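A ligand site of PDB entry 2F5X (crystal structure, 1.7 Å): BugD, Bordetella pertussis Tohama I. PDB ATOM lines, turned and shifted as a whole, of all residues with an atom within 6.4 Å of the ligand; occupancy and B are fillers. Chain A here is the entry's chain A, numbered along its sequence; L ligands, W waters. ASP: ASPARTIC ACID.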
ATOM      1  N   VAL A  23      -6.530  16.294 -19.409  1.00  0.00           N
ATOM      2  CA  VAL A  23      -5.815  16.790 -20.584  1.00  0.00           C
ATOM      3  C   VAL A  23      -6.867  17.507 -21.430  1.00  0.00           C
ATOM      4  O   VAL A  23      -7.800  16.860 -21.907  1.00  0.00           O
ATOM      5  CB  VAL A  23      -5.220  15.606 -21.378  1.00  0.00           C
ATOM      6  CG1 VAL A  23      -4.720  16.037 -22.755  1.00  0.00           C
ATOM      7  CG2 VAL A  23      -4.095  14.962 -20.575  1.00  0.00           C
ATOM      8  N   PRO A  24      -6.781  18.832 -21.586  1.00  0.00           N
ATOM      9  CA  PRO A  24      -7.815  19.594 -22.321  1.00  0.00           C
ATOM     10  C   PRO A  24      -7.856  19.423 -23.840  1.00  0.00           C
ATOM     11  O   PRO A  24      -8.206  20.372 -24.561  1.00  0.00           O
ATOM     12  CB  PRO A  24      -7.490  21.045 -21.950  1.00  0.00           C
ATOM     13  CG  PRO A  24      -6.733  20.917 -20.612  1.00  0.00           C
ATOM     14  CD  PRO A  24      -5.814  19.739 -20.938  1.00  0.00           C
ATOM     15  N   PHE A  25      -7.534  18.228 -24.333  1.00  0.00           N
ATOM     16  CA  PHE A  25      -7.511  17.944 -25.767  1.00  0.00           C
ATOM     17  C   PHE A  25      -7.861  16.499 -26.035  1.00  0.00           C
ATOM     18  O   PHE A  25      -7.795  15.661 -25.144  1.00  0.00           O
ATOM     19  CB  PHE A  25      -6.120  18.229 -26.349  1.00  0.00           C
ATOM     20  CG  PHE A  25      -5.731  19.675 -26.267  1.00  0.00           C
ATOM     21  CD1 PHE A  25      -6.265  20.610 -27.162  1.00  0.00           C
ATOM     22  CD2 PHE A  25      -4.864  20.112 -25.290  1.00  0.00           C
ATOM     23  CE1 PHE A  25      -5.928  21.945 -27.076  1.00  0.00           C
ATOM     24  CE2 PHE A  25      -4.512  21.463 -25.194  1.00  0.00           C
ATOM     25  CZ  PHE A  25      -5.033  22.379 -26.098  1.00  0.00           C
ATOM     26  N   ALA A  26      -8.216  16.228 -27.293  1.00  0.00           N
ATOM     27  CA  ALA A  26      -8.606  14.896 -27.716  1.00  0.00           C
ATOM     28  C   ALA A  26      -7.516  13.860 -27.425  1.00  0.00           C
ATOM     29  O   ALA A  26      -6.320  14.155 -27.531  1.00  0.00           O
ATOM     30  CB  ALA A  26      -8.945  14.915 -29.201  1.00  0.00           C
ATOM     31  N   GLY A  29      -3.354  12.650 -29.065  1.00  0.00           N
ATOM     32  CA  GLY A  29      -2.551  13.761 -29.550  1.00  0.00           C
ATOM     33  C   GLY A  29      -1.346  14.031 -28.663  1.00  0.00           C
ATOM     34  O   GLY A  29      -1.006  13.222 -27.795  1.00  0.00           O
ATOM     35  N   PRO A  30      -0.691  15.161 -28.876  1.00  0.00           N
ATOM     36  CA  PRO A  30       0.613  15.425 -28.236  1.00  0.00           C
ATOM     37  C   PRO A  30       0.545  15.491 -26.716  1.00  0.00           C
ATOM     38  O   PRO A  30       1.342  14.847 -26.031  1.00  0.00           O
ATOM     39  CB  PRO A  30       1.051  16.760 -28.859  1.00  0.00           C
ATOM     40  CG  PRO A  30      -0.202  17.362 -29.472  1.00  0.00           C
ATOM     41  CD  PRO A  30      -1.113  16.232 -29.789  1.00  0.00           C
ATOM     42  N   THR A  31      -0.393  16.248 -26.171  1.00  0.00           N
ATOM     43  CA  THR A  31      -0.485  16.393 -24.718  1.00  0.00           C
ATOM     44  C   THR A  31      -0.943  15.084 -24.076  1.00  0.00           C
ATOM     45  O   THR A  31      -0.491  14.730 -22.989  1.00  0.00           O
ATOM     46  CB  THR A  31      -1.392  17.567 -24.361  1.00  0.00           C
ATOM     47  OG1 THR A  31      -0.835  18.757 -24.910  1.00  0.00           O
ATOM     48  CG2 THR A  31      -1.393  17.829 -22.841  1.00  0.00           C
ATOM     49  N   ASP A  32      -1.849  14.384 -24.742  1.00  0.00           N
ATOM     50  CA  ASP A  32      -2.279  13.057 -24.272  1.00  0.00           C
ATOM     51  C   ASP A  32      -1.101  12.070 -24.203  1.00  0.00           C
ATOM     52  O   ASP A  32      -0.992  11.270 -23.257  1.00  0.00           O
ATOM     53  CB  ASP A  32      -3.379  12.506 -25.193  1.00  0.00           C
ATOM     54  CG  ASP A  32      -4.011  11.256 -24.649  1.00  0.00           C
ATOM     55  OD1 ASP A  32      -4.530  11.297 -23.500  1.00  0.00           O
ATOM     56  OD2 ASP A  32      -4.012  10.186 -25.285  1.00  0.00           O
ATOM     57  N   GLY A  59      -9.791  25.352 -27.555  1.00  0.00           N
ATOM     58  CA  GLY A  59      -8.340  25.488 -27.485  1.00  0.00           C
ATOM     59  C   GLY A  59      -7.714  25.067 -26.170  1.00  0.00           C
ATOM     60  O   GLY A  59      -6.607  25.490 -25.850  1.00  0.00           O
ATOM     61  N   MET A  80      -1.513  20.735 -18.682  1.00  0.00           N
ATOM     62  CA  MET A  80      -1.802  21.692 -19.742  1.00  0.00           C
ATOM     63  C   MET A  80      -0.507  22.352 -20.188  1.00  0.00           C
ATOM     64  O   MET A  80       0.454  22.431 -19.426  1.00  0.00           O
ATOM     65  CB  MET A  80      -2.835  22.719 -19.256  1.00  0.00           C
ATOM     66  CG  MET A  80      -3.318  23.747 -20.299  1.00  0.00           C
ATOM     67  SD  MET A  80      -3.919  22.982 -21.997  1.00  0.00           S
ATOM     68  CE  MET A  80      -4.084  24.672 -22.993  1.00  0.00           C
ATOM     69  N   HIS A  81      -0.493  22.842 -21.425  1.00  0.00           N
ATOM     70  CA  HIS A  81       0.691  23.441 -22.007  1.00  0.00           C
ATOM     71  C   HIS A  81       0.617  24.962 -22.065  1.00  0.00           C
ATOM     72  O   HIS A  81      -0.266  25.568 -21.448  1.00  0.00           O
ATOM     73  CB  HIS A  81       0.979  22.809 -23.381  1.00  0.00           C
ATOM     74  CG  HIS A  81      -0.096  22.988 -24.399  1.00  0.00           C
ATOM     75  ND1 HIS A  81      -0.688  24.214 -24.659  1.00  0.00           N
ATOM     76  CD2 HIS A  81      -0.665  22.109 -25.264  1.00  0.00           C
ATOM     77  CE1 HIS A  81      -1.573  24.069 -25.636  1.00  0.00           C
ATOM     78  NE2 HIS A  81      -1.575  22.806 -26.020  1.00  0.00           N
ATOM     79  N   MET A 113       7.940  22.451 -32.109  1.00  0.00           N
ATOM     80  CA  MET A 113       6.930  22.224 -33.130  1.00  0.00           C
ATOM     81  C   MET A 113       7.523  22.061 -34.538  1.00  0.00           C
ATOM     82  O   MET A 113       8.655  22.501 -34.815  1.00  0.00           O
ATOM     83  CB  MET A 113       5.869  23.320 -33.072  1.00  0.00           C
ATOM     84  CG  MET A 113       5.228  23.421 -31.668  1.00  0.00           C
ATOM     85  SD  MET A 113       3.898  24.787 -31.605  1.00  0.00           S
ATOM     86  CE  MET A 113       2.476  23.773 -32.546  1.00  0.00           C
ATOM     87  N   ASN A 144      -5.796  23.971 -36.821  1.00  0.00           N
ATOM     88  CA  ASN A 144      -5.303  24.098 -35.447  1.00  0.00           C
ATOM     89  C   ASN A 144      -6.265  23.429 -34.459  1.00  0.00           C
ATOM     90  O   ASN A 144      -7.286  22.872 -34.860  1.00  0.00           O
ATOM     91  CB  ASN A 144      -4.993  25.553 -35.059  1.00  0.00           C
ATOM     92  CG  ASN A 144      -6.241  26.447 -35.022  1.00  0.00           C
ATOM     93  OD1 ASN A 144      -7.341  26.000 -34.690  1.00  0.00           O
ATOM     94  ND2 ASN A 144      -6.057  27.721 -35.359  1.00  0.00           N
ATOM     95  N   ALA A 145      -5.917  23.473 -33.171  1.00  0.00           N
ATOM     96  CA  ALA A 145      -6.729  22.824 -32.151  1.00  0.00           C
ATOM     97  C   ALA A 145      -7.551  23.849 -31.347  1.00  0.00           C
ATOM     98  O   ALA A 145      -7.829  23.663 -30.152  1.00  0.00           O
ATOM     99  CB  ALA A 145      -5.845  21.932 -31.225  1.00  0.00           C
ATOM    100  N   GLY A 148      -6.241  29.420 -28.582  1.00  0.00           N
ATOM    101  CA  GLY A 148      -5.639  29.028 -27.302  1.00  0.00           C
ATOM    102  C   GLY A 148      -4.721  27.821 -27.389  1.00  0.00           C
ATOM    103  O   GLY A 148      -3.968  27.565 -26.447  1.00  0.00           O
ATOM    104  N   ALA A 149      -4.754  27.086 -28.496  1.00  0.00           N
ATOM    105  CA  ALA A 149      -3.931  25.885 -28.652  1.00  0.00           C
ATOM    106  C   ALA A 149      -2.495  26.235 -29.032  1.00  0.00           C
ATOM    107  O   ALA A 149      -2.214  27.361 -29.441  1.00  0.00           O
ATOM    108  CB  ALA A 149      -4.546  24.945 -29.702  1.00  0.00           C
ATOM    109  N   ALA A 150      -1.591  25.258 -28.905  1.00  0.00           N
ATOM    110  CA  ALA A 150      -0.211  25.411 -29.355  1.00  0.00           C
ATOM    111  C   ALA A 150      -0.185  25.612 -30.866  1.00  0.00           C
ATOM    112  O   ALA A 150       0.507  26.482 -31.394  1.00  0.00           O
ATOM    113  CB  ALA A 150       0.609  24.181 -28.957  1.00  0.00           C
ATOM    114  N   SER A 151      -0.971  24.797 -31.563  1.00  0.00           N
ATOM    115  CA  SER A 151      -1.073  24.872 -33.006  1.00  0.00           C
ATOM    116  C   SER A 151      -1.705  26.190 -33.446  1.00  0.00           C
ATOM    117  O   SER A 151      -1.458  26.655 -34.547  1.00  0.00           O
ATOM    118  CB  SER A 151      -1.863  23.676 -33.566  1.00  0.00           C
ATOM    119  OG  SER A 151      -3.124  23.541 -32.921  1.00  0.00           O
ATOM    120  N   HIS A 152      -2.532  26.780 -32.578  1.00  0.00           N
ATOM    121  CA  HIS A 152      -3.109  28.099 -32.847  1.00  0.00           C
ATOM    122  C   HIS A 152      -2.054  29.195 -32.747  1.00  0.00           C
ATOM    123  O   HIS A 152      -1.969  30.065 -33.632  1.00  0.00           O
ATOM    124  CB  HIS A 152      -4.284  28.397 -31.911  1.00  0.00           C
ATOM    125  CG  HIS A 152      -4.728  29.825 -31.963  1.00  0.00           C
ATOM    126  ND1 HIS A 152      -4.419  30.732 -30.967  1.00  0.00           N
ATOM    127  CD2 HIS A 152      -5.430  30.517 -32.891  1.00  0.00           C
ATOM    128  CE1 HIS A 152      -4.912  31.915 -31.286  1.00  0.00           C
ATOM    129  NE2 HIS A 152      -5.528  31.806 -32.457  1.00  0.00           N
ATOM    130  N   LYS A 172     -10.681  19.674 -31.843  1.00  0.00           N
ATOM    131  CA  LYS A 172     -10.586  19.518 -30.393  1.00  0.00           C
ATOM    132  C   LYS A 172      -9.207  19.059 -29.926  1.00  0.00           C
ATOM    133  O   LYS A 172      -8.995  18.775 -28.749  1.00  0.00           O
ATOM    134  CB  LYS A 172     -11.669  18.557 -29.884  1.00  0.00           C
ATOM    135  CG  LYS A 172     -13.060  19.176 -29.861  1.00  0.00           C
ATOM    136  CD  LYS A 172     -14.114  18.146 -29.463  1.00  0.00           C
ATOM    137  CE  LYS A 172     -15.447  18.800 -29.134  1.00  0.00           C
ATOM    138  NZ  LYS A 172     -15.807  19.932 -30.043  1.00  0.00           N
ATOM    139  N   GLY A 173      -8.279  18.946 -30.866  1.00  0.00           N
ATOM    140  CA  GLY A 173      -6.923  18.523 -30.582  1.00  0.00           C
ATOM    141  C   GLY A 173      -6.212  18.297 -31.899  1.00  0.00           C
ATOM    142  O   GLY A 173      -6.857  18.260 -32.942  1.00  0.00           O
ATOM    143  N   THR A 174      -4.897  18.149 -31.870  1.00  0.00           N
ATOM    144  CA  THR A 174      -4.217  17.836 -33.146  1.00  0.00           C
ATOM    145  C   THR A 174      -4.225  16.353 -33.511  1.00  0.00           C
ATOM    146  O   THR A 174      -3.770  16.016 -34.598  1.00  0.00           O
ATOM    147  CB  THR A 174      -2.792  18.408 -33.228  1.00  0.00           C
ATOM    148  OG1 THR A 174      -2.050  17.998 -32.063  1.00  0.00           O
ATOM    149  CG2 THR A 174      -2.842  19.943 -33.183  1.00  0.00           C
ATOM    150  N   ALA A 175      -4.735  15.485 -32.650  1.00  0.00           N
ATOM    151  CA  ALA A 175      -5.008  14.112 -33.073  1.00  0.00           C
ATOM    152  C   ALA A 175      -6.096  14.079 -34.181  1.00  0.00           C
ATOM    153  O   ALA A 175      -5.834  13.555 -35.275  1.00  0.00           O
ATOM    154  CB  ALA A 175      -5.356  13.191 -31.874  1.00  0.00           C
ATOM    155  N   PRO A 176      -7.300  14.611 -33.938  1.00  0.00           N
ATOM    156  CA  PRO A 176      -8.302  14.702 -35.016  1.00  0.00           C
ATOM    157  C   PRO A 176      -7.826  15.552 -36.198  1.00  0.00           C
ATOM    158  O   PRO A 176      -8.141  15.224 -37.346  1.00  0.00           O
ATOM    159  CB  PRO A 176      -9.526  15.339 -34.352  1.00  0.00           C
ATOM    160  CG  PRO A 176      -9.073  15.868 -33.062  1.00  0.00           C
ATOM    161  CD  PRO A 176      -7.846  15.090 -32.655  1.00  0.00           C
ATOM    162  N   CYS A 190       0.877  23.487 -37.992  1.00  0.00           N
ATOM    163  CA  CYS A 190       2.022  23.481 -37.080  1.00  0.00           C
ATOM    164  C   CYS A 190       1.633  22.669 -35.872  1.00  0.00           C
ATOM    165  O   CYS A 190       0.587  22.935 -35.271  1.00  0.00           O
ATOM    166  CB  CYS A 190       2.353  24.894 -36.632  1.00  0.00           C
ATOM    167  SG  CYS A 190       3.943  25.081 -35.757  1.00  0.00           S
ATOM    168  N   ASP A 191       2.447  21.691 -35.508  1.00  0.00           N
ATOM    169  CA  ASP A 191       2.054  20.740 -34.447  1.00  0.00           C
ATOM    170  C   ASP A 191       3.311  20.265 -33.707  1.00  0.00           C
ATOM    171  O   ASP A 191       4.438  20.416 -34.214  1.00  0.00           O
ATOM    172  CB  ASP A 191       1.240  19.608 -35.111  1.00  0.00           C
ATOM    173  CG  ASP A 191       0.640  18.604 -34.120  1.00  0.00           C
ATOM    174  OD1 ASP A 191       0.525  18.848 -32.888  1.00  0.00           O
ATOM    175  OD2 ASP A 191       0.213  17.507 -34.540  1.00  0.00           O
ATOM    176  N   GLN A 192       3.125  19.744 -32.502  1.00  0.00           N
ATOM    177  CA  GLN A 192       4.254  19.350 -31.640  1.00  0.00           C
ATOM    178  C   GLN A 192       4.867  18.036 -32.061  1.00  0.00           C
ATOM    179  O   GLN A 192       4.152  17.168 -32.571  1.00  0.00           O
ATOM    180  CB  GLN A 192       3.786  19.254 -30.198  1.00  0.00           C
ATOM    181  CG  GLN A 192       3.343  20.590 -29.615  1.00  0.00           C
ATOM    182  CD  GLN A 192       2.425  20.377 -28.447  1.00  0.00           C
ATOM    183  OE1 GLN A 192       1.209  20.557 -28.553  1.00  0.00           O
ATOM    184  NE2 GLN A 192       2.992  19.970 -27.336  1.00  0.00           N
ATOM    185  N   ILE A 237       6.734  24.564 -26.584  1.00  0.00           N
ATOM    186  CA  ILE A 237       5.484  24.345 -25.861  1.00  0.00           C
ATOM    187  C   ILE A 237       5.783  23.678 -24.531  1.00  0.00           C
ATOM    188  O   ILE A 237       5.850  22.439 -24.430  1.00  0.00           O
ATOM    189  CB  ILE A 237       4.503  23.547 -26.749  1.00  0.00           C
ATOM    190  CG1 ILE A 237       4.205  24.331 -28.044  1.00  0.00           C
ATOM    191  CG2 ILE A 237       3.194  23.234 -26.007  1.00  0.00           C
ATOM    192  CD1 ILE A 237       3.612  25.739 -27.859  1.00  0.00           C
ATOM    193  N   HIS A 239       4.936  22.489 -20.776  1.00  0.00           N
ATOM    194  CA  HIS A 239       3.764  21.879 -20.151  1.00  0.00           C
ATOM    195  C   HIS A 239       3.923  22.019 -18.628  1.00  0.00           C
ATOM    196  O   HIS A 239       5.038  21.914 -18.100  1.00  0.00           O
ATOM    197  CB  HIS A 239       3.689  20.379 -20.476  1.00  0.00           C
ATOM    198  CG  HIS A 239       3.181  20.069 -21.862  1.00  0.00           C
ATOM    199  ND1 HIS A 239       3.786  20.535 -23.007  1.00  0.00           N
ATOM    200  CD2 HIS A 239       2.141  19.290 -22.264  1.00  0.00           C
ATOM    201  CE1 HIS A 239       3.127  20.079 -24.060  1.00  0.00           C
ATOM    202  NE2 HIS A 239       2.131  19.325 -23.639  1.00  0.00           N
HETATM  203  N   ASP L   1      -1.478  20.003 -27.411  1.00  0.00           N
HETATM  204  CA  ASP L   1      -2.787  19.883 -28.116  1.00  0.00           C
HETATM  205  C   ASP L   1      -3.278  18.439 -28.144  1.00  0.00           C
HETATM  206  O   ASP L   1      -4.074  18.061 -29.021  1.00  0.00           O
HETATM  207  CB  ASP L   1      -2.673  20.417 -29.542  1.00  0.00           C
HETATM  208  CG  ASP L   1      -2.431  21.898 -29.582  1.00  0.00           C
HETATM  209  OD1 ASP L   1      -2.095  22.404 -30.686  1.00  0.00           O
HETATM  210  OD2 ASP L   1      -2.542  22.635 -28.575  1.00  0.00           O
HETATM  211  OXT ASP L   1      -2.863  17.672 -27.279  1.00  0.00           O
HETATM  212  O   HOH W   1      -3.660  15.146 -26.895  1.00  0.00           O
HETATM  213  O   HOH W   2      -5.333  15.781 -29.730  1.00  0.00           O
HETATM  214  O   HOH W   3       0.233  21.217 -31.341  1.00  0.00           O
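The backbone NH (N) of Thr 174 is in hydrogen-bond range of an oxygen (O) of the ligand, 3.0 Å away. The side-chain hydroxyl (OG1) of Thr 31 is in hydrogen-bond range of a nitrogen (N) of the ligand, 2.9 Å away. OE1 of Gln 192 lies within hydrogen-bond range of N of the ligand. The backbone NH (N) of Ala 150 sits at hydrogen-bond distance from an oxygen (OD2) of the ligand. N of Ser 151 is in hydrogen-bond range of OD1 of the ligand, at 2.8 Å. An oxygen (OXT) of the ligand sits at hydrogen-bond distance from the backbone NH (N) of Thr 31 (3.1 Å). The side-chain hydroxyl of Ser 151 sits at hydrogen-bond distance from an oxygen (OD1) of the ligand (2.7 Å). A ring nitrogen (NE2) of His 81 is in hydrogen-bond range of an oxygen (OD2) of the ligand (2.7 Å).
The backbone NH (N) of Ala 145 lies within hydrogen-bond range of the side-chain hydroxyl (OG) of Ser 151 (2.8 Å). The side-chain hydroxyl of Thr 31 sits at hydrogen-bond distance from a ring nitrogen (NE2) of His 239 (3.3 Å). OG1 of Thr 174 is in hydrogen-bond range of OD1 of Asp 191 (2.8 Å).
Merely in contact with the ligand: Ala 149, Gly 173, Phe 25, Pro 30 and Ala 145. 11 residues have an atom within 4 Å of the ligand: Phe 25, Pro 30, Thr 31, His 81, Ala 145, Ala 149, Ala 150, Ser 151, Gly 173, Thr 174 and Gln 192. The nearest printed residue that does not touch the ligand is Gly 29 (4.2 Å).
Water W1 lies within hydrogen-bond range of OXT of the ligand (2.7 Å), O of Ala 26 (2.9 Å), N of Asp 32 (2.9 Å) and N of Gly 29 (3.3 Å). Water W3 lies within hydrogen-bond range of an oxygen (OD1) of the ligand, the side-chain carboxylate (OD1) of Asp 191 and the side-chain amide oxygen (OE1) of Gln 192. Water W2 lies within hydrogen-bond range of O of the ligand (2.7 Å), O of Ala 26 (2.9 Å), N of Ala 175 (3.0 Å) and N of Thr 174 (3.2 Å).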
